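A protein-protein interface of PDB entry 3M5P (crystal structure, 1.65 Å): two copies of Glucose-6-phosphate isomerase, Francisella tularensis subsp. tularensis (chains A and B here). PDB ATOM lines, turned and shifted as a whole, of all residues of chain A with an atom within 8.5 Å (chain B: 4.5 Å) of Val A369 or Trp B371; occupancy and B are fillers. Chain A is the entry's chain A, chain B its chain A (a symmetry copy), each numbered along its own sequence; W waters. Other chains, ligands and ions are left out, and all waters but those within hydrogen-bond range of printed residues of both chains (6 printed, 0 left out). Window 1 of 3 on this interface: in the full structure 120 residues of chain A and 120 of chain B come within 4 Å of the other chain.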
ATOM      1  N   SER A 319     -18.036  -6.902 -11.339  1.00  0.00           N
ATOM      2  CA  SER A 319     -17.707  -7.607 -10.121  1.00  0.00           C
ATOM      3  C   SER A 319     -16.248  -8.082 -10.132  1.00  0.00           C
ATOM      4  O   SER A 319     -15.634  -8.228  -9.055  1.00  0.00           O
ATOM      5  CB  SER A 319     -18.723  -8.705  -9.779  1.00  0.00           C
ATOM      6  OG  SER A 319     -18.786  -9.772 -10.708  1.00  0.00           O
ATOM      7  N   SER A 324     -16.848  -5.073  -7.005  1.00  0.00           N
ATOM      8  CA  SER A 324     -18.175  -4.899  -6.417  1.00  0.00           C
ATOM      9  C   SER A 324     -18.736  -6.256  -5.963  1.00  0.00           C
ATOM     10  O   SER A 324     -18.381  -7.314  -6.489  1.00  0.00           O
ATOM     11  CB  SER A 324     -19.111  -4.203  -7.397  1.00  0.00           C
ATOM     12  OG  SER A 324     -19.109  -4.848  -8.661  1.00  0.00           O
ATOM     13  N   GLN A 325     -19.570  -6.200  -4.932  1.00  0.00           N
ATOM     14  CA  GLN A 325     -20.061  -7.395  -4.246  1.00  0.00           C
ATOM     15  C   GLN A 325     -21.580  -7.406  -4.175  1.00  0.00           C
ATOM     16  O   GLN A 325     -22.164  -8.252  -3.506  1.00  0.00           O
ATOM     17  CB  GLN A 325     -19.448  -7.454  -2.840  1.00  0.00           C
ATOM     18  CG  GLN A 325     -17.921  -7.597  -2.846  1.00  0.00           C
ATOM     19  CD  GLN A 325     -17.303  -7.559  -1.479  1.00  0.00           C
ATOM     20  OE1 GLN A 325     -17.871  -8.002  -0.519  1.00  0.00           O
ATOM     21  NE2 GLN A 325     -16.145  -6.948  -1.385  1.00  0.00           N
ATOM     22  N   SER A 326     -22.220  -6.503  -4.922  1.00  0.00           N
ATOM     23  CA  SER A 326     -23.675  -6.533  -5.095  1.00  0.00           C
ATOM     24  C   SER A 326     -24.098  -5.840  -6.385  1.00  0.00           C
ATOM     25  O   SER A 326     -23.310  -5.136  -7.017  1.00  0.00           O
ATOM     26  CB  SER A 326     -24.430  -5.877  -3.893  1.00  0.00           C
ATOM     27  OG  SER A 326     -24.408  -4.480  -3.986  1.00  0.00           O
ATOM     28  N   GLN A 327     -25.356  -6.090  -6.762  1.00  0.00           N
ATOM     29  CA  GLN A 327     -26.021  -5.480  -7.889  1.00  0.00           C
ATOM     30  C   GLN A 327     -27.413  -5.091  -7.418  1.00  0.00           C
ATOM     31  O   GLN A 327     -28.045  -5.859  -6.696  1.00  0.00           O
ATOM     32  CB  GLN A 327     -26.202  -6.484  -9.030  1.00  0.00           C
ATOM     33  CG  GLN A 327     -24.959  -6.812  -9.836  1.00  0.00           C
ATOM     34  CD  GLN A 327     -25.296  -7.853 -10.896  1.00  0.00           C
ATOM     35  OE1 GLN A 327     -25.569  -7.510 -12.062  1.00  0.00           O
ATOM     36  NE2 GLN A 327     -25.325  -9.117 -10.484  1.00  0.00           N
ATOM     37  N   ALA A 328     -27.877  -3.908  -7.837  1.00  0.00           N
ATOM     38  CA  ALA A 328     -29.196  -3.396  -7.493  1.00  0.00           C
ATOM     39  C   ALA A 328     -30.143  -3.563  -8.702  1.00  0.00           C
ATOM     40  O   ALA A 328     -29.792  -3.199  -9.836  1.00  0.00           O
ATOM     41  CB  ALA A 328     -29.090  -1.905  -7.083  1.00  0.00           C
ATOM     42  N   LEU A 329     -31.350  -4.034  -8.432  1.00  0.00           N
ATOM     43  CA  LEU A 329     -32.412  -4.225  -9.441  1.00  0.00           C
ATOM     44  C   LEU A 329     -33.625  -3.443  -8.935  1.00  0.00           C
ATOM     45  O   LEU A 329     -34.076  -3.670  -7.814  1.00  0.00           O
ATOM     46  CB  LEU A 329     -32.700  -5.717  -9.533  1.00  0.00           C
ATOM     47  CG  LEU A 329     -33.854  -6.193 -10.391  1.00  0.00           C
ATOM     48  CD1 LEU A 329     -33.722  -5.644 -11.836  1.00  0.00           C
ATOM     49  CD2 LEU A 329     -33.954  -7.701 -10.379  1.00  0.00           C
ATOM     50  N   VAL A 340     -37.517  -8.908  -7.445  1.00  0.00           N
ATOM     51  CA  VAL A 340     -36.200  -9.003  -6.827  1.00  0.00           C
ATOM     52  C   VAL A 340     -36.120 -10.292  -5.999  1.00  0.00           C
ATOM     53  O   VAL A 340     -35.168 -11.043  -6.116  1.00  0.00           O
ATOM     54  CB  VAL A 340     -35.868  -7.789  -5.997  1.00  0.00           C
ATOM     55  CG1 VAL A 340     -34.590  -8.031  -5.158  1.00  0.00           C
ATOM     56  CG2 VAL A 340     -35.751  -6.531  -6.905  1.00  0.00           C
ATOM     57  N   LEU A 343     -35.594 -13.270  -8.319  1.00  0.00           N
ATOM     58  CA  LEU A 343     -34.286 -13.307  -8.975  1.00  0.00           C
ATOM     59  C   LEU A 343     -33.167 -13.507  -7.957  1.00  0.00           C
ATOM     60  O   LEU A 343     -32.122 -14.035  -8.316  1.00  0.00           O
ATOM     61  CB  LEU A 343     -34.067 -12.099  -9.881  1.00  0.00           C
ATOM     62  CG  LEU A 343     -34.883 -12.147 -11.201  1.00  0.00           C
ATOM     63  CD1 LEU A 343     -34.579 -10.891 -11.996  1.00  0.00           C
ATOM     64  CD2 LEU A 343     -34.710 -13.492 -12.041  1.00  0.00           C
ATOM     65  N   GLN A 344     -33.377 -13.153  -6.692  1.00  0.00           N
ATOM     66  CA  GLN A 344     -32.388 -13.503  -5.670  1.00  0.00           C
ATOM     67  C   GLN A 344     -32.136 -14.989  -5.619  1.00  0.00           C
ATOM     68  O   GLN A 344     -30.981 -15.387  -5.524  1.00  0.00           O
ATOM     69  CB  GLN A 344     -32.818 -13.039  -4.281  1.00  0.00           C
ATOM     70  CG  GLN A 344     -32.659 -11.606  -4.091  1.00  0.00           C
ATOM     71  CD  GLN A 344     -33.032 -11.170  -2.684  1.00  0.00           C
ATOM     72  OE1 GLN A 344     -33.942 -11.774  -2.050  1.00  0.00           O
ATOM     73  NE2 GLN A 344     -32.329 -10.133  -2.169  1.00  0.00           N
ATOM     74  N   ASP A 347     -30.501 -16.122  -9.157  1.00  0.00           N
ATOM     75  CA  ASP A 347     -29.130 -15.660  -9.324  1.00  0.00           C
ATOM     76  C   ASP A 347     -28.222 -16.255  -8.224  1.00  0.00           C
ATOM     77  O   ASP A 347     -27.290 -17.020  -8.526  1.00  0.00           O
ATOM     78  CB  ASP A 347     -29.151 -14.137  -9.343  1.00  0.00           C
ATOM     79  CG  ASP A 347     -27.821 -13.512  -9.657  1.00  0.00           C
ATOM     80  OD1 ASP A 347     -26.799 -14.217  -9.656  1.00  0.00           O
ATOM     81  OD2 ASP A 347     -27.843 -12.272  -9.921  1.00  0.00           O
ATOM     82  N   MET A 348     -28.524 -15.991  -6.955  1.00  0.00           N
ATOM     83  CA  MET A 348     -27.597 -16.313  -5.877  1.00  0.00           C
ATOM     84  C   MET A 348     -27.549 -17.793  -5.601  1.00  0.00           C
ATOM     85  O   MET A 348     -26.486 -18.298  -5.281  1.00  0.00           O
ATOM     86  CB  MET A 348     -27.975 -15.538  -4.607  1.00  0.00           C
ATOM     87  CG  MET A 348     -27.925 -14.019  -4.833  1.00  0.00           C
ATOM     88  SD  MET A 348     -28.486 -13.012  -3.283  1.00  0.00           S
ATOM     89  CE  MET A 348     -27.304 -13.388  -2.220  1.00  0.00           C
ATOM     90  N   GLY A 352     -23.681 -18.587  -6.387  1.00  0.00           N
ATOM     91  CA  GLY A 352     -22.987 -18.553  -5.126  1.00  0.00           C
ATOM     92  C   GLY A 352     -22.252 -19.863  -4.922  1.00  0.00           C
ATOM     93  O   GLY A 352     -22.686 -20.693  -4.159  1.00  0.00           O
ATOM     94  N   GLN A 365     -13.731 -14.015  -7.513  1.00  0.00           N
ATOM     95  CA  GLN A 365     -15.062 -13.914  -6.943  1.00  0.00           C
ATOM     96  C   GLN A 365     -16.095 -14.447  -7.964  1.00  0.00           C
ATOM     97  O   GLN A 365     -15.948 -14.221  -9.176  1.00  0.00           O
ATOM     98  CB  GLN A 365     -15.344 -12.462  -6.647  1.00  0.00           C
ATOM     99  CG  GLN A 365     -16.592 -12.208  -5.809  1.00  0.00           C
ATOM    100  CD  GLN A 365     -16.774 -10.754  -5.526  1.00  0.00           C
ATOM    101  OE1 GLN A 365     -16.445 -10.274  -4.414  1.00  0.00           O
ATOM    102  NE2 GLN A 365     -17.286 -10.005  -6.530  1.00  0.00           N
ATOM    103  N   THR A 366     -17.137 -15.114  -7.482  1.00  0.00           N
ATOM    104  CA  THR A 366     -18.216 -15.577  -8.341  1.00  0.00           C
ATOM    105  C   THR A 366     -19.485 -14.749  -8.078  1.00  0.00           C
ATOM    106  O   THR A 366     -19.415 -13.504  -8.075  1.00  0.00           O
ATOM    107  CB  THR A 366     -18.379 -17.107  -8.204  1.00  0.00           C
ATOM    108  OG1 THR A 366     -18.630 -17.403  -6.835  1.00  0.00           O
ATOM    109  CG2 THR A 366     -17.085 -17.831  -8.703  1.00  0.00           C
ATOM    110  N   GLY A 367     -20.631 -15.383  -7.812  1.00  0.00           N
ATOM    111  CA  GLY A 367     -21.891 -14.651  -7.722  1.00  0.00           C
ATOM    112  C   GLY A 367     -21.900 -13.650  -6.592  1.00  0.00           C
ATOM    113  O   GLY A 367     -21.359 -13.925  -5.507  1.00  0.00           O
ATOM    114  N   VAL A 368     -22.493 -12.491  -6.859  1.00  0.00           N
ATOM    115  CA  VAL A 368     -22.578 -11.418  -5.875  1.00  0.00           C
ATOM    116  C   VAL A 368     -24.049 -11.304  -5.378  1.00  0.00           C
ATOM    117  O   VAL A 368     -24.964 -12.001  -5.842  1.00  0.00           O
ATOM    118  CB  VAL A 368     -22.037 -10.071  -6.462  1.00  0.00           C
ATOM    119  CG1 VAL A 368     -20.562 -10.243  -7.011  1.00  0.00           C
ATOM    120  CG2 VAL A 368     -22.963  -9.475  -7.489  1.00  0.00           C
ATOM    121  N   VAL A 369     -24.244 -10.470  -4.377  1.00  0.00           N
ATOM    122  CA  VAL A 369     -25.541 -10.251  -3.795  1.00  0.00           C
ATOM    123  C   VAL A 369     -26.442  -9.491  -4.788  1.00  0.00           C
ATOM    124  O   VAL A 369     -26.063  -8.453  -5.325  1.00  0.00           O
ATOM    125  CB  VAL A 369     -25.439  -9.469  -2.475  1.00  0.00           C
ATOM    126  CG1 VAL A 369     -26.872  -9.076  -1.888  1.00  0.00           C
ATOM    127  CG2 VAL A 369     -24.601 -10.243  -1.422  1.00  0.00           C
ATOM    128  N   LEU A 370     -27.640  -9.999  -5.001  1.00  0.00           N
ATOM    129  CA  LEU A 370     -28.668  -9.298  -5.760  1.00  0.00           C
ATOM    130  C   LEU A 370     -29.693  -8.723  -4.772  1.00  0.00           C
ATOM    131  O   LEU A 370     -30.181  -9.425  -3.921  1.00  0.00           O
ATOM    132  CB  LEU A 370     -29.355 -10.218  -6.764  1.00  0.00           C
ATOM    133  CG  LEU A 370     -30.344  -9.527  -7.718  1.00  0.00           C
ATOM    134  CD1 LEU A 370     -29.728  -8.505  -8.678  1.00  0.00           C
ATOM    135  CD2 LEU A 370     -31.118 -10.614  -8.513  1.00  0.00           C
ATOM    136  N   TRP A 371     -29.987  -7.437  -4.904  1.00  0.00           N
ATOM    137  CA  TRP A 371     -30.915  -6.741  -4.019  1.00  0.00           C
ATOM    138  C   TRP A 371     -31.601  -5.615  -4.809  1.00  0.00           C
ATOM    139  O   TRP A 371     -31.266  -5.379  -5.968  1.00  0.00           O
ATOM    140  CB  TRP A 371     -30.213  -6.237  -2.753  1.00  0.00           C
ATOM    141  CG  TRP A 371     -29.261  -5.152  -3.059  1.00  0.00           C
ATOM    142  CD1 TRP A 371     -27.994  -5.278  -3.564  1.00  0.00           C
ATOM    143  CD2 TRP A 371     -29.500  -3.740  -2.917  1.00  0.00           C
ATOM    144  NE1 TRP A 371     -27.451  -4.041  -3.754  1.00  0.00           N
ATOM    145  CE2 TRP A 371     -28.348  -3.080  -3.364  1.00  0.00           C
ATOM    146  CE3 TRP A 371     -30.563  -2.988  -2.427  1.00  0.00           C
ATOM    147  CZ2 TRP A 371     -28.228  -1.694  -3.359  1.00  0.00           C
ATOM    148  CZ3 TRP A 371     -30.460  -1.602  -2.443  1.00  0.00           C
ATOM    149  CH2 TRP A 371     -29.307  -0.968  -2.926  1.00  0.00           C
ATOM    150  N   GLY A 372     -32.561  -4.933  -4.187  1.00  0.00           N
ATOM    151  CA  GLY A 372     -33.133  -3.758  -4.791  1.00  0.00           C
ATOM    152  C   GLY A 372     -34.479  -3.461  -4.191  1.00  0.00           C
ATOM    153  O   GLY A 372     -34.726  -3.722  -2.995  1.00  0.00           O
ATOM    154  N   ILE A 393     -21.870  -0.063  -7.180  1.00  0.00           N
ATOM    155  CA  ILE A 393     -23.050  -0.929  -7.323  1.00  0.00           C
ATOM    156  C   ILE A 393     -23.643  -0.742  -8.720  1.00  0.00           C
ATOM    157  O   ILE A 393     -24.221   0.311  -9.022  1.00  0.00           O
ATOM    158  CB  ILE A 393     -24.145  -0.642  -6.240  1.00  0.00           C
ATOM    159  CG1 ILE A 393     -23.573  -0.660  -4.793  1.00  0.00           C
ATOM    160  CG2 ILE A 393     -25.328  -1.625  -6.421  1.00  0.00           C
ATOM    161  CD1 ILE A 393     -24.449   0.048  -3.751  1.00  0.00           C
ATOM    162  N   PRO A 394     -23.518  -1.758  -9.592  1.00  0.00           N
ATOM    163  CA  PRO A 394     -24.231  -1.710 -10.863  1.00  0.00           C
ATOM    164  C   PRO A 394     -25.742  -1.722 -10.614  1.00  0.00           C
ATOM    165  O   PRO A 394     -26.207  -2.346  -9.646  1.00  0.00           O
ATOM    166  CB  PRO A 394     -23.810  -3.012 -11.571  1.00  0.00           C
ATOM    167  CG  PRO A 394     -22.585  -3.476 -10.846  1.00  0.00           C
ATOM    168  CD  PRO A 394     -22.704  -2.977  -9.464  1.00  0.00           C
ATOM    169  N   SER B 326     -21.777  -5.496   2.097  1.00  0.00           N
ATOM    170  CA  SER B 326     -23.172  -5.726   2.487  1.00  0.00           C
ATOM    171  C   SER B 326     -23.264  -6.467   3.816  1.00  0.00           C
ATOM    172  O   SER B 326     -22.276  -7.008   4.312  1.00  0.00           O
ATOM    173  CB  SER B 326     -23.967  -6.524   1.403  1.00  0.00           C
ATOM    174  OG  SER B 326     -23.681  -7.893   1.473  1.00  0.00           O
ATOM    175  N   GLN B 327     -24.475  -6.442   4.381  1.00  0.00           N
ATOM    176  CA  GLN B 327     -24.843  -7.147   5.586  1.00  0.00           C
ATOM    177  C   GLN B 327     -26.196  -7.786   5.325  1.00  0.00           C
ATOM    178  O   GLN B 327     -27.057  -7.156   4.716  1.00  0.00           O
ATOM    179  CB  GLN B 327     -25.027  -6.176   6.756  1.00  0.00           C
ATOM    180  CG  GLN B 327     -23.758  -5.618   7.370  1.00  0.00           C
ATOM    181  CD  GLN B 327     -24.114  -4.641   8.483  1.00  0.00           C
ATOM    182  OE1 GLN B 327     -24.143  -5.012   9.672  1.00  0.00           O
ATOM    183  NE2 GLN B 327     -24.431  -3.409   8.098  1.00  0.00           N
ATOM    184  N   ALA B 328     -26.371  -9.028   5.793  1.00  0.00           N
ATOM    185  CA  ALA B 328     -27.612  -9.774   5.644  1.00  0.00           C
ATOM    186  C   ALA B 328     -28.382  -9.764   6.983  1.00  0.00           C
ATOM    187  O   ALA B 328     -27.804 -10.042   8.047  1.00  0.00           O
ATOM    188  CB  ALA B 328     -27.302 -11.227   5.202  1.00  0.00           C
ATOM    189  N   LEU B 329     -29.681  -9.521   6.904  1.00  0.00           N
ATOM    190  CA  LEU B 329     -30.596  -9.512   8.063  1.00  0.00           C
ATOM    191  C   LEU B 329     -31.710 -10.507   7.734  1.00  0.00           C
ATOM    192  O   LEU B 329     -32.358 -10.380   6.697  1.00  0.00           O
ATOM    193  CB  LEU B 329     -31.131  -8.095   8.218  1.00  0.00           C
ATOM    194  CG  LEU B 329     -32.210  -7.823   9.247  1.00  0.00           C
ATOM    195  CD1 LEU B 329     -31.766  -8.320  10.648  1.00  0.00           C
ATOM    196  CD2 LEU B 329     -32.580  -6.358   9.271  1.00  0.00           C
ATOM    197  N   VAL B 340     -36.702  -5.853   6.921  1.00  0.00           N
ATOM    198  CA  VAL B 340     -35.532  -5.530   6.114  1.00  0.00           C
ATOM    199  C   VAL B 340     -35.810  -4.260   5.302  1.00  0.00           C
ATOM    200  O   VAL B 340     -35.004  -3.348   5.284  1.00  0.00           O
ATOM    201  CB  VAL B 340     -35.114  -6.676   5.226  1.00  0.00           C
ATOM    202  CG1 VAL B 340     -34.042  -6.220   4.209  1.00  0.00           C
ATOM    203  CG2 VAL B 340     -34.638  -7.880   6.091  1.00  0.00           C
ATOM    204  N   GLN B 344     -33.556  -0.942   5.614  1.00  0.00           N
ATOM    205  CA  GLN B 344     -32.810  -0.433   4.460  1.00  0.00           C
ATOM    206  C   GLN B 344     -32.841   1.072   4.392  1.00  0.00           C
ATOM    207  O   GLN B 344     -31.805   1.671   4.129  1.00  0.00           O
ATOM    208  CB  GLN B 344     -33.354  -0.986   3.145  1.00  0.00           C
ATOM    209  CG  GLN B 344     -32.969  -2.370   2.913  1.00  0.00           C
ATOM    210  CD  GLN B 344     -33.465  -2.885   1.573  1.00  0.00           C
ATOM    211  OE1 GLN B 344     -34.554  -2.464   1.091  1.00  0.00           O
ATOM    212  NE2 GLN B 344     -32.671  -3.786   0.943  1.00  0.00           N
ATOM    213  N   VAL B 369     -24.542  -1.967   1.916  1.00  0.00           N
ATOM    214  CA  VAL B 369     -25.851  -2.423   1.533  1.00  0.00           C
ATOM    215  C   VAL B 369     -26.441  -3.320   2.640  1.00  0.00           C
ATOM    216  O   VAL B 369     -25.804  -4.266   3.099  1.00  0.00           O
ATOM    217  CB  VAL B 369     -25.808  -3.193   0.202  1.00  0.00           C
ATOM    218  CG1 VAL B 369     -27.219  -3.845  -0.168  1.00  0.00           C
ATOM    219  CG2 VAL B 369     -25.292  -2.295  -0.954  1.00  0.00           C
ATOM    220  N   LEU B 370     -27.665  -3.033   3.037  1.00  0.00           N
ATOM    221  CA  LEU B 370     -28.424  -3.898   3.932  1.00  0.00           C
ATOM    222  C   LEU B 370     -29.465  -4.662   3.101  1.00  0.00           C
ATOM    223  O   LEU B 370     -30.194  -4.071   2.342  1.00  0.00           O
ATOM    224  CB  LEU B 370     -29.107  -3.103   5.041  1.00  0.00           C
ATOM    225  CG  LEU B 370     -29.800  -3.947   6.122  1.00  0.00           C
ATOM    226  CD1 LEU B 370     -28.873  -4.829   6.965  1.00  0.00           C
ATOM    227  CD2 LEU B 370     -30.629  -3.007   7.040  1.00  0.00           C
ATOM    228  N   TRP B 371     -29.499  -5.977   3.258  1.00  0.00           N
ATOM    229  CA  TRP B 371     -30.408  -6.842   2.514  1.00  0.00           C
ATOM    230  C   TRP B 371     -30.753  -8.062   3.382  1.00  0.00           C
ATOM    231  O   TRP B 371     -30.212  -8.217   4.474  1.00  0.00           O
ATOM    232  CB  TRP B 371     -29.826  -7.228   1.149  1.00  0.00           C
ATOM    233  CG  TRP B 371     -28.658  -8.120   1.295  1.00  0.00           C
ATOM    234  CD1 TRP B 371     -27.372  -7.760   1.605  1.00  0.00           C
ATOM    235  CD2 TRP B 371     -28.657  -9.553   1.170  1.00  0.00           C
ATOM    236  NE1 TRP B 371     -26.595  -8.877   1.694  1.00  0.00           N
ATOM    237  CE2 TRP B 371     -27.351  -9.988   1.430  1.00  0.00           C
ATOM    238  CE3 TRP B 371     -29.629 -10.491   0.836  1.00  0.00           C
ATOM    239  CZ2 TRP B 371     -26.987 -11.331   1.388  1.00  0.00           C
ATOM    240  CZ3 TRP B 371     -29.277 -11.835   0.816  1.00  0.00           C
ATOM    241  CH2 TRP B 371     -27.969 -12.244   1.112  1.00  0.00           C
ATOM    242  N   GLY B 372     -31.657  -8.915   2.902  1.00  0.00           N
ATOM    243  CA  GLY B 372     -31.911 -10.164   3.569  1.00  0.00           C
ATOM    244  C   GLY B 372     -33.256 -10.707   3.174  1.00  0.00           C
ATOM    245  O   GLY B 372     -33.723 -10.512   2.032  1.00  0.00           O
ATOM    246  N   PHE B 382     -31.439 -17.868  -1.045  1.00  0.00           N
ATOM    247  CA  PHE B 382     -30.107 -17.301  -1.115  1.00  0.00           C
ATOM    248  C   PHE B 382     -29.159 -17.757  -0.033  1.00  0.00           C
ATOM    249  O   PHE B 382     -27.947 -17.433  -0.113  1.00  0.00           O
ATOM    250  CB  PHE B 382     -30.166 -15.765  -1.112  1.00  0.00           C
ATOM    251  CG  PHE B 382     -30.943 -15.207   0.061  1.00  0.00           C
ATOM    252  CD1 PHE B 382     -30.360 -15.179   1.308  1.00  0.00           C
ATOM    253  CD2 PHE B 382     -32.249 -14.769  -0.077  1.00  0.00           C
ATOM    254  CE1 PHE B 382     -31.057 -14.728   2.423  1.00  0.00           C
ATOM    255  CE2 PHE B 382     -32.957 -14.289   1.020  1.00  0.00           C
ATOM    256  CZ  PHE B 382     -32.338 -14.277   2.295  1.00  0.00           C
ATOM    257  N   LEU B 386     -24.731 -17.668   1.038  1.00  0.00           N
ATOM    258  CA  LEU B 386     -24.154 -17.441   2.363  1.00  0.00           C
ATOM    259  C   LEU B 386     -23.267 -18.605   2.792  1.00  0.00           C
ATOM    260  O   LEU B 386     -22.256 -18.391   3.487  1.00  0.00           O
ATOM    261  CB  LEU B 386     -25.249 -17.215   3.406  1.00  0.00           C
ATOM    262  CG  LEU B 386     -26.157 -15.990   3.220  1.00  0.00           C
ATOM    263  CD1 LEU B 386     -27.174 -15.938   4.372  1.00  0.00           C
ATOM    264  CD2 LEU B 386     -25.398 -14.667   3.103  1.00  0.00           C
ATOM    265  N   ILE B 393     -19.938 -11.735   4.188  1.00  0.00           N
ATOM    266  CA  ILE B 393     -21.219 -11.094   4.519  1.00  0.00           C
ATOM    267  C   ILE B 393     -21.552 -11.367   5.986  1.00  0.00           C
ATOM    268  O   ILE B 393     -21.879 -12.503   6.357  1.00  0.00           O
ATOM    269  CB  ILE B 393     -22.395 -11.590   3.608  1.00  0.00           C
ATOM    270  CG1 ILE B 393     -22.059 -11.489   2.093  1.00  0.00           C
ATOM    271  CG2 ILE B 393     -23.694 -10.833   3.979  1.00  0.00           C
ATOM    272  CD1 ILE B 393     -22.940 -12.358   1.184  1.00  0.00           C
HETATM  273  O   HOH W   1     -19.869  -8.135   0.983  1.00  0.00           O
HETATM  274  O   HOH W   2     -33.106  -8.618   0.263  1.00  0.00           O
HETATM  275  O   HOH W   3     -33.519  -5.449  -1.365  1.00  0.00           O
HETATM  276  O   HOH W   4     -36.175  -3.463  -0.691  1.00  0.00           O
HETATM  277  O   HOH W   5     -35.431 -11.059  -0.033  1.00  0.00           O
HETATM  278  O   HOH W   6     -22.086  -7.953  -0.592  1.00  0.00           O
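Ser A326 touches Val B369, and with the chains exchanged Val A369 touches Ser B326. Val A369 touches Trp B371, and with the chains exchanged Trp A371 touches Val B369. Val A369 touches Ile B393, and with the chains exchanged Ile A393 touches Val B369.
Among the printed residues, pairs that only touch across the chains: Ser A326 with Val B369 (3.8 Å), Gln A344 with Phe B382 (3.97 Å), Met A348 with Trp B371 (3.6 Å), Met A348 with Phe B382 (3.9 Å), Val A369 with Ser B326 (3.8 Å), Val A369 with Trp B371 (3.5 Å), Val A369 with Ile B393 (3.7 Å), Trp A371 with Val B369 (3.5 Å) and Ile A393 with Val B369 (3.7 Å).
Water W1 bridges OE1 of Gln A325 (2.5 Å) and N of Ser B326 (3.4 Å). Water W5 lies within hydrogen-bond range of OE1 of Gln A344 (2.6 Å) and O of Gly B372 (2.7 Å). Water W4 lies within hydrogen-bond range of the side-chain amide oxygen of Gln B344 (2.6 Å) and the backbone carbonyl oxygen of Gly A372 (2.7 Å). Water W6 bridges the side-chain hydroxyl of Ser B326 and the backbone carbonyl oxygen of Gln A325. Water W3 lies within hydrogen-bond range of the backbone carbonyl oxygen of Gly A372 and the side-chain amide nitrogen of Gln B344. Water W2 lies within hydrogen-bond range of O of Gly B372 (2.7 Å) and NE2 of Gln A344 (3.0 Å).
Val A369 touches just these residues of chain B: Ser B326 (3.8 Å), Trp B371 (3.5 Å) and Ile B393 (3.7 Å). Trp B371 touches two residues of chain A. No residue of chain A comes within 4 Å of Gly B372. Of the printed residues of chain A, Phe B382 touches Gln A344 (3.97 Å) and Met A348 (3.9 Å). Printed residues of chain B within 4 Å of Trp A371: Val B369 (3.5 Å). Of the printed residues of chain A, Ile B393 touches Val A369 (3.7 Å). Of the printed residues of chain B, Gln A344 touches Phe B382 (3.97 Å). Of the printed residues of chain B, Ser A326 touches Val B369. Val A368 touches none of the printed residues of chain B. The nearest printed residue of chain B that does not touch Val A369 is Val B369 (5.5 Å). The nearest printed residue of chain A that does not touch Trp B371 is Trp A371 (4.04 Å). The nearest printed residue of chain A that does not touch Ile B393 is Met A348 (5.6 Å).
O of Gln A325 is in hydrogen-bond range of N of Val A369, 3.2 Å away. The side-chain hydroxyl of Ser A326 lies within hydrogen-bond range of the indole nitrogen of Trp A371 (3.1 Å). The backbone carbonyl oxygen (O) of Gln B327 sits at hydrogen-bond distance from the backbone NH (N) of Trp B371. O of Val A369 lies within hydrogen-bond range of N of Gln A327 (2.9 Å). N of Leu A370 is in hydrogen-bond range of SD of Met A348 (3.6 Å). N of Gln B327 lies within hydrogen-bond range of O of Val B369 (2.9 Å).
Hydrophobic or aromatic side chains of chain B that line the printed part of chain A: Val B369, Trp B371, Phe B382 and Ile B393. Printed residues of chain A that touch a printed residue of chain B: Ser A326, Gln A344, Met A348, Val A369, Trp A371 and Ile A393. Hydrophobic or aromatic side chains of chain A that line the printed part of chain B: Met A348, Val A369, Trp A371 and Ile A393. Among the printed residues, no Asp or Glu carboxylate lies within 4 Å of a Lys or Arg side-chain nitrogen of the other chain.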
